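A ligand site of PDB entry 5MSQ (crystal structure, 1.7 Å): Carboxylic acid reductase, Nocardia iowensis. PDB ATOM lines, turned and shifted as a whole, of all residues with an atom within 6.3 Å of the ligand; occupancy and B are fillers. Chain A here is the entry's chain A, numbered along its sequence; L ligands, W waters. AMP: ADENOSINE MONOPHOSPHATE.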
ATOM      1  N   THR A 255     -10.774   1.634 -15.333  1.00  0.00           N
ATOM      2  CA  THR A 255     -11.066   0.304 -14.805  1.00  0.00           C
ATOM      3  C   THR A 255     -12.410   0.351 -14.081  1.00  0.00           C
ATOM      4  O   THR A 255     -12.808   1.397 -13.571  1.00  0.00           O
ATOM      5  CB  THR A 255      -9.927  -0.190 -13.858  1.00  0.00           C
ATOM      6  OG1 THR A 255     -10.184  -1.533 -13.436  1.00  0.00           O
ATOM      7  CG2 THR A 255      -9.783   0.718 -12.636  1.00  0.00           C
ATOM      8  N   HIS A 300      -5.685  -1.495 -21.718  1.00  0.00           N
ATOM      9  CA  HIS A 300      -5.433  -2.312 -20.541  1.00  0.00           C
ATOM     10  C   HIS A 300      -3.960  -2.362 -20.240  1.00  0.00           C
ATOM     11  O   HIS A 300      -3.142  -2.368 -21.146  1.00  0.00           O
ATOM     12  CB  HIS A 300      -5.966  -3.728 -20.750  1.00  0.00           C
ATOM     13  CG  HIS A 300      -6.038  -4.536 -19.491  1.00  0.00           C
ATOM     14  ND1 HIS A 300      -4.985  -5.290 -19.016  1.00  0.00           N
ATOM     15  CD2 HIS A 300      -7.050  -4.720 -18.613  1.00  0.00           C
ATOM     16  CE1 HIS A 300      -5.349  -5.900 -17.902  1.00  0.00           C
ATOM     17  NE2 HIS A 300      -6.595  -5.561 -17.632  1.00  0.00           N
ATOM     18  N   ILE A 301      -3.614  -2.421 -18.957  1.00  0.00           N
ATOM     19  CA  ILE A 301      -2.221  -2.465 -18.549  1.00  0.00           C
ATOM     20  C   ILE A 301      -1.458  -3.628 -19.211  1.00  0.00           C
ATOM     21  O   ILE A 301      -0.306  -3.476 -19.628  1.00  0.00           O
ATOM     22  CB  ILE A 301      -2.113  -2.562 -17.013  1.00  0.00           C
ATOM     23  CG1 ILE A 301      -0.645  -2.598 -16.577  1.00  0.00           C
ATOM     24  CG2 ILE A 301      -2.821  -3.801 -16.476  1.00  0.00           C
ATOM     25  CD1 ILE A 301       0.133  -1.391 -16.979  1.00  0.00           C
ATOM     26  N   VAL A 393       0.284 -16.860 -17.621  1.00  0.00           N
ATOM     27  CA  VAL A 393      -1.156 -16.630 -17.649  1.00  0.00           C
ATOM     28  C   VAL A 393      -1.508 -15.627 -16.551  1.00  0.00           C
ATOM     29  O   VAL A 393      -0.895 -15.626 -15.486  1.00  0.00           O
ATOM     30  CB  VAL A 393      -1.952 -17.948 -17.443  1.00  0.00           C
ATOM     31  CG1 VAL A 393      -1.644 -18.562 -16.091  1.00  0.00           C
ATOM     32  CG2 VAL A 393      -3.476 -17.703 -17.599  1.00  0.00           C
ATOM     33  N   GLY A 394      -2.472 -14.752 -16.808  1.00  0.00           N
ATOM     34  CA  GLY A 394      -2.901 -13.809 -15.781  1.00  0.00           C
ATOM     35  C   GLY A 394      -4.214 -13.118 -16.102  1.00  0.00           C
ATOM     36  O   GLY A 394      -4.870 -13.461 -17.087  1.00  0.00           O
ATOM     37  N   SER A 395      -4.575 -12.155 -15.245  1.00  0.00           N
ATOM     38  CA  SER A 395      -5.776 -11.320 -15.376  1.00  0.00           C
ATOM     39  C   SER A 395      -7.042 -11.960 -14.813  1.00  0.00           C
ATOM     40  O   SER A 395      -8.009 -11.259 -14.517  1.00  0.00           O
ATOM     41  CB  SER A 395      -6.037 -10.932 -16.838  1.00  0.00           C
ATOM     42  OG  SER A 395      -6.813 -11.917 -17.506  1.00  0.00           O
ATOM     43  N   ALA A 396      -7.034 -13.274 -14.658  1.00  0.00           N
ATOM     44  CA  ALA A 396      -8.205 -13.966 -14.144  1.00  0.00           C
ATOM     45  C   ALA A 396      -7.793 -15.355 -13.689  1.00  0.00           C
ATOM     46  O   ALA A 396      -6.710 -15.809 -14.022  1.00  0.00           O
ATOM     47  CB  ALA A 396      -9.322 -14.036 -15.206  1.00  0.00           C
ATOM     48  N   PRO A 397      -8.653 -16.018 -12.896  1.00  0.00           N
ATOM     49  CA  PRO A 397      -8.199 -17.294 -12.350  1.00  0.00           C
ATOM     50  C   PRO A 397      -8.115 -18.389 -13.420  1.00  0.00           C
ATOM     51  O   PRO A 397      -8.958 -18.431 -14.310  1.00  0.00           O
ATOM     52  CB  PRO A 397      -9.274 -17.624 -11.301  1.00  0.00           C
ATOM     53  CG  PRO A 397     -10.448 -16.756 -11.616  1.00  0.00           C
ATOM     54  CD  PRO A 397      -9.925 -15.543 -12.324  1.00  0.00           C
ATOM     55  N   LEU A 398      -7.090 -19.221 -13.333  1.00  0.00           N
ATOM     56  CA  LEU A 398      -6.992 -20.425 -14.155  1.00  0.00           C
ATOM     57  C   LEU A 398      -7.030 -21.623 -13.209  1.00  0.00           C
ATOM     58  O   LEU A 398      -6.211 -21.700 -12.290  1.00  0.00           O
ATOM     59  CB  LEU A 398      -5.718 -20.440 -15.000  1.00  0.00           C
ATOM     60  CG  LEU A 398      -5.721 -21.508 -16.107  1.00  0.00           C
ATOM     61  CD1 LEU A 398      -6.686 -21.103 -17.215  1.00  0.00           C
ATOM     62  CD2 LEU A 398      -4.334 -21.716 -16.681  1.00  0.00           C
ATOM     63  N   ASP A 416       1.853 -18.286 -13.345  1.00  0.00           N
ATOM     64  CA  ASP A 416       0.612 -17.581 -13.001  1.00  0.00           C
ATOM     65  C   ASP A 416       0.995 -16.229 -12.446  1.00  0.00           C
ATOM     66  O   ASP A 416       1.642 -16.166 -11.395  1.00  0.00           O
ATOM     67  CB  ASP A 416      -0.202 -18.394 -11.987  1.00  0.00           C
ATOM     68  CG  ASP A 416      -1.569 -17.786 -11.679  1.00  0.00           C
ATOM     69  OD1 ASP A 416      -1.860 -16.645 -12.096  1.00  0.00           O
ATOM     70  OD2 ASP A 416      -2.365 -18.460 -10.992  1.00  0.00           O
ATOM     71  N   GLY A 417       0.634 -15.153 -13.138  1.00  0.00           N
ATOM     72  CA  GLY A 417       0.941 -13.809 -12.654  1.00  0.00           C
ATOM     73  C   GLY A 417      -0.308 -13.079 -12.183  1.00  0.00           C
ATOM     74  O   GLY A 417      -1.275 -12.922 -12.942  1.00  0.00           O
ATOM     75  N   TYR A 418      -0.297 -12.653 -10.922  1.00  0.00           N
ATOM     76  CA  TYR A 418      -1.388 -11.869 -10.372  1.00  0.00           C
ATOM     77  C   TYR A 418      -0.969 -10.416 -10.214  1.00  0.00           C
ATOM     78  O   TYR A 418       0.106 -10.127  -9.693  1.00  0.00           O
ATOM     79  CB  TYR A 418      -1.858 -12.433  -9.034  1.00  0.00           C
ATOM     80  CG  TYR A 418      -2.687 -11.447  -8.237  1.00  0.00           C
ATOM     81  CD1 TYR A 418      -4.056 -11.346  -8.439  1.00  0.00           C
ATOM     82  CD2 TYR A 418      -2.102 -10.608  -7.293  1.00  0.00           C
ATOM     83  CE1 TYR A 418      -4.838 -10.449  -7.712  1.00  0.00           C
ATOM     84  CE2 TYR A 418      -2.878  -9.692  -6.566  1.00  0.00           C
ATOM     85  CZ  TYR A 418      -4.233  -9.617  -6.789  1.00  0.00           C
ATOM     86  OH  TYR A 418      -5.015  -8.720  -6.076  1.00  0.00           O
ATOM     87  N   GLY A 419      -1.840  -9.510 -10.633  1.00  0.00           N
ATOM     88  CA  GLY A 419      -1.630  -8.085 -10.483  1.00  0.00           C
ATOM     89  C   GLY A 419      -2.911  -7.341 -10.776  1.00  0.00           C
ATOM     90  O   GLY A 419      -3.937  -7.959 -11.061  1.00  0.00           O
ATOM     91  N   SER A 420      -2.880  -6.016 -10.712  1.00  0.00           N
ATOM     92  CA  SER A 420      -4.069  -5.218 -11.019  1.00  0.00           C
ATOM     93  C   SER A 420      -3.672  -3.858 -11.567  1.00  0.00           C
ATOM     94  O   SER A 420      -2.535  -3.455 -11.421  1.00  0.00           O
ATOM     95  CB  SER A 420      -4.928  -5.006  -9.776  1.00  0.00           C
ATOM     96  OG  SER A 420      -4.204  -4.265  -8.795  1.00  0.00           O
ATOM     97  N   THR A 421      -4.636  -3.154 -12.140  1.00  0.00           N
ATOM     98  CA  THR A 421      -4.416  -1.790 -12.605  1.00  0.00           C
ATOM     99  C   THR A 421      -3.944  -0.903 -11.457  1.00  0.00           C
ATOM    100  O   THR A 421      -3.043  -0.090 -11.628  1.00  0.00           O
ATOM    101  CB  THR A 421      -5.716  -1.210 -13.221  1.00  0.00           C
ATOM    102  OG1 THR A 421      -6.088  -2.013 -14.341  1.00  0.00           O
ATOM    103  CG2 THR A 421      -5.523   0.237 -13.680  1.00  0.00           C
ATOM    104  N   GLU A 422      -4.528  -1.085 -10.279  1.00  0.00           N
ATOM    105  CA  GLU A 422      -4.218  -0.241  -9.118  1.00  0.00           C
ATOM    106  C   GLU A 422      -2.873  -0.562  -8.454  1.00  0.00           C
ATOM    107  O   GLU A 422      -2.152   0.334  -8.026  1.00  0.00           O
ATOM    108  CB  GLU A 422      -5.326  -0.350  -8.058  1.00  0.00           C
ATOM    109  CG  GLU A 422      -6.655   0.240  -8.477  1.00  0.00           C
ATOM    110  CD  GLU A 422      -7.551  -0.728  -9.238  1.00  0.00           C
ATOM    111  OE1 GLU A 422      -7.072  -1.798  -9.704  1.00  0.00           O
ATOM    112  OE2 GLU A 422      -8.750  -0.418  -9.356  1.00  0.00           O
ATOM    113  N   LEU A 428       2.078 -11.016  -7.596  1.00  0.00           N
ATOM    114  CA  LEU A 428       2.405 -12.421  -7.375  1.00  0.00           C
ATOM    115  C   LEU A 428       2.840 -13.074  -8.659  1.00  0.00           C
ATOM    116  O   LEU A 428       2.287 -12.800  -9.727  1.00  0.00           O
ATOM    117  CB  LEU A 428       1.216 -13.191  -6.810  1.00  0.00           C
ATOM    118  CG  LEU A 428       0.710 -12.892  -5.410  1.00  0.00           C
ATOM    119  CD1 LEU A 428      -0.628 -13.585  -5.173  1.00  0.00           C
ATOM    120  CD2 LEU A 428       1.736 -13.339  -4.400  1.00  0.00           C
ATOM    121  N   THR A 493      -7.146  -4.477  -1.934  1.00  0.00           N
ATOM    122  CA  THR A 493      -7.285  -5.073  -3.266  1.00  0.00           C
ATOM    123  C   THR A 493      -8.708  -5.491  -3.612  1.00  0.00           C
ATOM    124  O   THR A 493      -9.042  -5.624  -4.794  1.00  0.00           O
ATOM    125  CB  THR A 493      -6.407  -6.322  -3.430  1.00  0.00           C
ATOM    126  OG1 THR A 493      -6.820  -7.327  -2.497  1.00  0.00           O
ATOM    127  CG2 THR A 493      -4.931  -5.974  -3.225  1.00  0.00           C
ATOM    128  N   GLY A 494      -9.525  -5.736  -2.598  1.00  0.00           N
ATOM    129  CA  GLY A 494     -10.829  -6.338  -2.814  1.00  0.00           C
ATOM    130  C   GLY A 494     -10.740  -7.809  -3.187  1.00  0.00           C
ATOM    131  O   GLY A 494     -11.726  -8.399  -3.613  1.00  0.00           O
ATOM    132  N   ASP A 495      -9.549  -8.399  -3.045  1.00  0.00           N
ATOM    133  CA  ASP A 495      -9.341  -9.802  -3.397  1.00  0.00           C
ATOM    134  C   ASP A 495      -9.065 -10.659  -2.184  1.00  0.00           C
ATOM    135  O   ASP A 495      -8.275 -10.275  -1.312  1.00  0.00           O
ATOM    136  CB  ASP A 495      -8.193  -9.936  -4.398  1.00  0.00           C
ATOM    137  CG  ASP A 495      -8.500  -9.270  -5.722  1.00  0.00           C
ATOM    138  OD1 ASP A 495      -9.680  -9.189  -6.093  1.00  0.00           O
ATOM    139  OD2 ASP A 495      -7.568  -8.818  -6.405  1.00  0.00           O
ATOM    140  N   TYR A 507      -4.511 -17.041  -4.666  1.00  0.00           N
ATOM    141  CA  TYR A 507      -5.668 -16.211  -4.951  1.00  0.00           C
ATOM    142  C   TYR A 507      -6.934 -17.053  -4.825  1.00  0.00           C
ATOM    143  O   TYR A 507      -6.990 -18.173  -5.338  1.00  0.00           O
ATOM    144  CB  TYR A 507      -5.539 -15.601  -6.350  1.00  0.00           C
ATOM    145  CG  TYR A 507      -6.736 -14.811  -6.834  1.00  0.00           C
ATOM    146  CD1 TYR A 507      -6.825 -13.437  -6.629  1.00  0.00           C
ATOM    147  CD2 TYR A 507      -7.762 -15.443  -7.528  1.00  0.00           C
ATOM    148  CE1 TYR A 507      -7.913 -12.724  -7.083  1.00  0.00           C
ATOM    149  CE2 TYR A 507      -8.851 -14.731  -7.996  1.00  0.00           C
ATOM    150  CZ  TYR A 507      -8.916 -13.374  -7.763  1.00  0.00           C
ATOM    151  OH  TYR A 507     -10.001 -12.673  -8.238  1.00  0.00           O
ATOM    152  N   ASP A 509     -10.687 -15.556  -4.770  1.00  0.00           N
ATOM    153  CA  ASP A 509     -11.628 -14.883  -5.668  1.00  0.00           C
ATOM    154  C   ASP A 509     -11.754 -13.432  -5.224  1.00  0.00           C
ATOM    155  O   ASP A 509     -11.227 -13.047  -4.177  1.00  0.00           O
ATOM    156  CB  ASP A 509     -12.995 -15.579  -5.657  1.00  0.00           C
ATOM    157  CG  ASP A 509     -13.743 -15.434  -6.987  1.00  0.00           C
ATOM    158  OD1 ASP A 509     -13.506 -14.465  -7.752  1.00  0.00           O
ATOM    159  OD2 ASP A 509     -14.599 -16.306  -7.268  1.00  0.00           O
ATOM    160  N   ARG A 510     -12.450 -12.617  -6.016  1.00  0.00           N
ATOM    161  CA  ARG A 510     -12.770 -11.261  -5.600  1.00  0.00           C
ATOM    162  C   ARG A 510     -13.807 -11.309  -4.476  1.00  0.00           C
ATOM    163  O   ARG A 510     -14.727 -12.117  -4.511  1.00  0.00           O
ATOM    164  CB  ARG A 510     -13.319 -10.443  -6.765  1.00  0.00           C
ATOM    165  CG  ARG A 510     -12.462 -10.475  -7.996  1.00  0.00           C
ATOM    166  CD  ARG A 510     -11.666  -9.198  -8.116  1.00  0.00           C
ATOM    167  NE  ARG A 510     -12.517  -8.034  -8.226  1.00  0.00           N
ATOM    168  CZ  ARG A 510     -12.292  -6.872  -7.607  1.00  0.00           C
ATOM    169  NH1 ARG A 510     -11.226  -6.693  -6.830  1.00  0.00           N
ATOM    170  NH2 ARG A 510     -13.157  -5.893  -7.800  1.00  0.00           N
ATOM    171  N   ILE A 614     -10.317  -7.683 -22.583  1.00  0.00           N
ATOM    172  CA  ILE A 614      -9.365  -8.784 -22.380  1.00  0.00           C
ATOM    173  C   ILE A 614     -10.091 -10.114 -22.132  1.00  0.00           C
ATOM    174  O   ILE A 614      -9.500 -11.056 -21.588  1.00  0.00           O
ATOM    175  CB  ILE A 614      -8.402  -8.496 -21.209  1.00  0.00           C
ATOM    176  CG1 ILE A 614      -9.160  -8.359 -19.887  1.00  0.00           C
ATOM    177  CG2 ILE A 614      -7.560  -7.245 -21.505  1.00  0.00           C
ATOM    178  CD1 ILE A 614      -8.254  -8.387 -18.656  1.00  0.00           C
ATOM    179  N   LYS A 616     -12.633 -11.102 -20.282  1.00  0.00           N
ATOM    180  CA  LYS A 616     -13.129 -11.469 -18.973  1.00  0.00           C
ATOM    181  C   LYS A 616     -14.645 -11.287 -18.959  1.00  0.00           C
ATOM    182  O   LYS A 616     -15.145 -10.366 -19.594  1.00  0.00           O
ATOM    183  CB  LYS A 616     -12.476 -10.599 -17.902  1.00  0.00           C
ATOM    184  CG  LYS A 616     -12.764 -11.010 -16.465  1.00  0.00           C
ATOM    185  CD  LYS A 616     -12.110 -10.047 -15.465  1.00  0.00           C
ATOM    186  CE  LYS A 616     -10.590 -10.104 -15.531  1.00  0.00           C
ATOM    187  NZ  LYS A 616      -9.935  -9.339 -14.395  1.00  0.00           N
HETATM  188  P   AMP L   1      -7.362  -5.486 -13.827  1.00  0.00           P
HETATM  189  O1P AMP L   1      -8.310  -5.191 -14.941  1.00  0.00           O
HETATM  190  O2P AMP L   1      -5.913  -5.680 -14.147  1.00  0.00           O
HETATM  191  O3P AMP L   1      -7.221  -4.275 -12.962  1.00  0.00           O
HETATM  192  O5' AMP L   1      -7.904  -6.756 -13.062  1.00  0.00           O
HETATM  193  C5' AMP L   1      -7.510  -6.987 -11.720  1.00  0.00           C
HETATM  194  C4' AMP L   1      -8.201  -8.200 -11.147  1.00  0.00           C
HETATM  195  O4' AMP L   1      -7.991  -9.356 -12.004  1.00  0.00           O
HETATM  196  C3' AMP L   1      -7.684  -8.649  -9.802  1.00  0.00           C
HETATM  197  O3' AMP L   1      -8.213  -7.852  -8.754  1.00  0.00           O
HETATM  198  C2' AMP L   1      -8.098 -10.123  -9.748  1.00  0.00           C
HETATM  199  O2' AMP L   1      -9.467 -10.260  -9.432  1.00  0.00           O
HETATM  200  C1' AMP L   1      -7.931 -10.534 -11.214  1.00  0.00           C
HETATM  201  N9  AMP L   1      -6.649 -11.220 -11.466  1.00  0.00           N
HETATM  202  C8  AMP L   1      -5.523 -10.693 -12.028  1.00  0.00           C
HETATM  203  N7  AMP L   1      -4.564 -11.600 -12.167  1.00  0.00           N
HETATM  204  C5  AMP L   1      -5.069 -12.810 -11.657  1.00  0.00           C
HETATM  205  C6  AMP L   1      -4.607 -14.143 -11.484  1.00  0.00           C
HETATM  206  N6  AMP L   1      -3.265 -14.534 -11.901  1.00  0.00           N
HETATM  207  N1  AMP L   1      -5.439 -15.028 -10.951  1.00  0.00           N
HETATM  208  C2  AMP L   1      -6.634 -14.715 -10.582  1.00  0.00           C
HETATM  209  N3  AMP L   1      -7.206 -13.535 -10.683  1.00  0.00           N
HETATM  210  C4  AMP L   1      -6.441 -12.556 -11.210  1.00  0.00           C
HETATM  211  O   HOH W   1      -4.183 -16.934 -13.928  1.00  0.00           O
HETATM  212  O   HOH W   2     -11.493 -10.038 -11.854  1.00  0.00           O
HETATM  213  O   HOH W   3      -8.737  -5.011  -9.310  1.00  0.00           O
HETATM  214  O   HOH W   4      -8.888  -3.276 -11.195  1.00  0.00           O
HETATM  215  O   HOH W   5     -10.117  -6.957 -15.488  1.00  0.00           O
HETATM  216  O   HOH W   6      -4.425 -17.508  -9.893  1.00  0.00           O
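O of Ala 396 lies close to N1 of the ligand (3.4 Å).
Gly 394 touches the ligand (CA to N6, 3.96 Å).
N of Pro 397 touches C2 of the ligand, 3.3 Å away.
Tyr 418 touches the ligand.
Gly 419 touches the ligand.
CA of Ser 420 touches O2P of the ligand (3.7 Å).
Arg 510 touches the ligand.
Hydrophobic or aromatic side chains that line the ligand: His 300, Pro 397, Tyr 418 and Tyr 507.
Of the 25 residues printed, 15 come within 4 Å of the ligand.
A nitrogen (N6) of the ligand sits at hydrogen-bond distance from the side-chain carboxylate of Asp 416 (2.5 Å).
An oxygen (O3') of the ligand lies within hydrogen-bond range of the side-chain carboxylate (OD2) of Asp 495, 2.6 Å away.
An oxygen (O2') of the ligand lies within hydrogen-bond range of the side-chain hydroxyl (OH) of Tyr 507 (2.7 Å).
A nitrogen (N6) of the ligand lies within hydrogen-bond range of the backbone carbonyl oxygen (O) of Gly 417 (2.8 Å).
The backbone NH (N) of Thr 421 is in hydrogen-bond range of an oxygen (O3P) of the ligand (2.9 Å).
O3P of the ligand is in hydrogen-bond range of OG1 of Thr 421.
The side-chain amino group (NZ) of Lys 616 sits at hydrogen-bond distance from an oxygen (O4') of the ligand, 3.1 Å away.
N7 of the ligand sits at hydrogen-bond distance from N of Ser 395 (3.1 Å).
O1P of the ligand is in hydrogen-bond range of NE2 of His 300, at 3.2 Å.
Water W5 bridges an oxygen (O1P) of the ligand and the side-chain amino group of Lys 616.
Water W4 lies within hydrogen-bond range of an oxygen (O3P) of the ligand (2.6 Å), the side-chain carboxylate (OE1) of Glu 422 (2.8 Å) and the side-chain hydroxyl (OG1) of Thr 255 (3.1 Å).
Water W6 lies within hydrogen-bond range of OD2 of Asp 416 and N1 of the ligand.
Water W2 bridges the side-chain amino group of Lys 616 (3.1 Å) and an oxygen (O2') of the ligand (3.2 Å).
Water W1 lies within hydrogen-bond range of O of Ala 396 (2.8 Å), OD1 of Asp 416 (3.0 Å) and N6 of the ligand (3.3 Å).
The side-chain carboxylate (OD1) of Asp 495 lies within salt-bridge range of the guanidinium group (NH1) of Arg 510 (3.0 Å).
The side-chain carboxylate of Asp 495 lies within hydrogen-bond range of the side-chain hydroxyl of Tyr 418, at 2.6 Å.
N of Asp 495 is in hydrogen-bond range of OG1 of Thr 493 (3.0 Å).
OH of Tyr 507 sits at hydrogen-bond distance from N of Arg 510 (3.3 Å).
N of Gly 417 lies within hydrogen-bond range of O of Val 393, at 2.8 Å.
NH1 of Arg 510 lies within hydrogen-bond range of O of Thr 493, 3.2 Å away.
NZ of Lys 616 lies within hydrogen-bond range of O of Ser 395 (2.7 Å).
The backbone carbonyl oxygen (O) of Leu 428 sits at hydrogen-bond distance from the backbone NH (N) of Tyr 418, 2.9 Å away.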
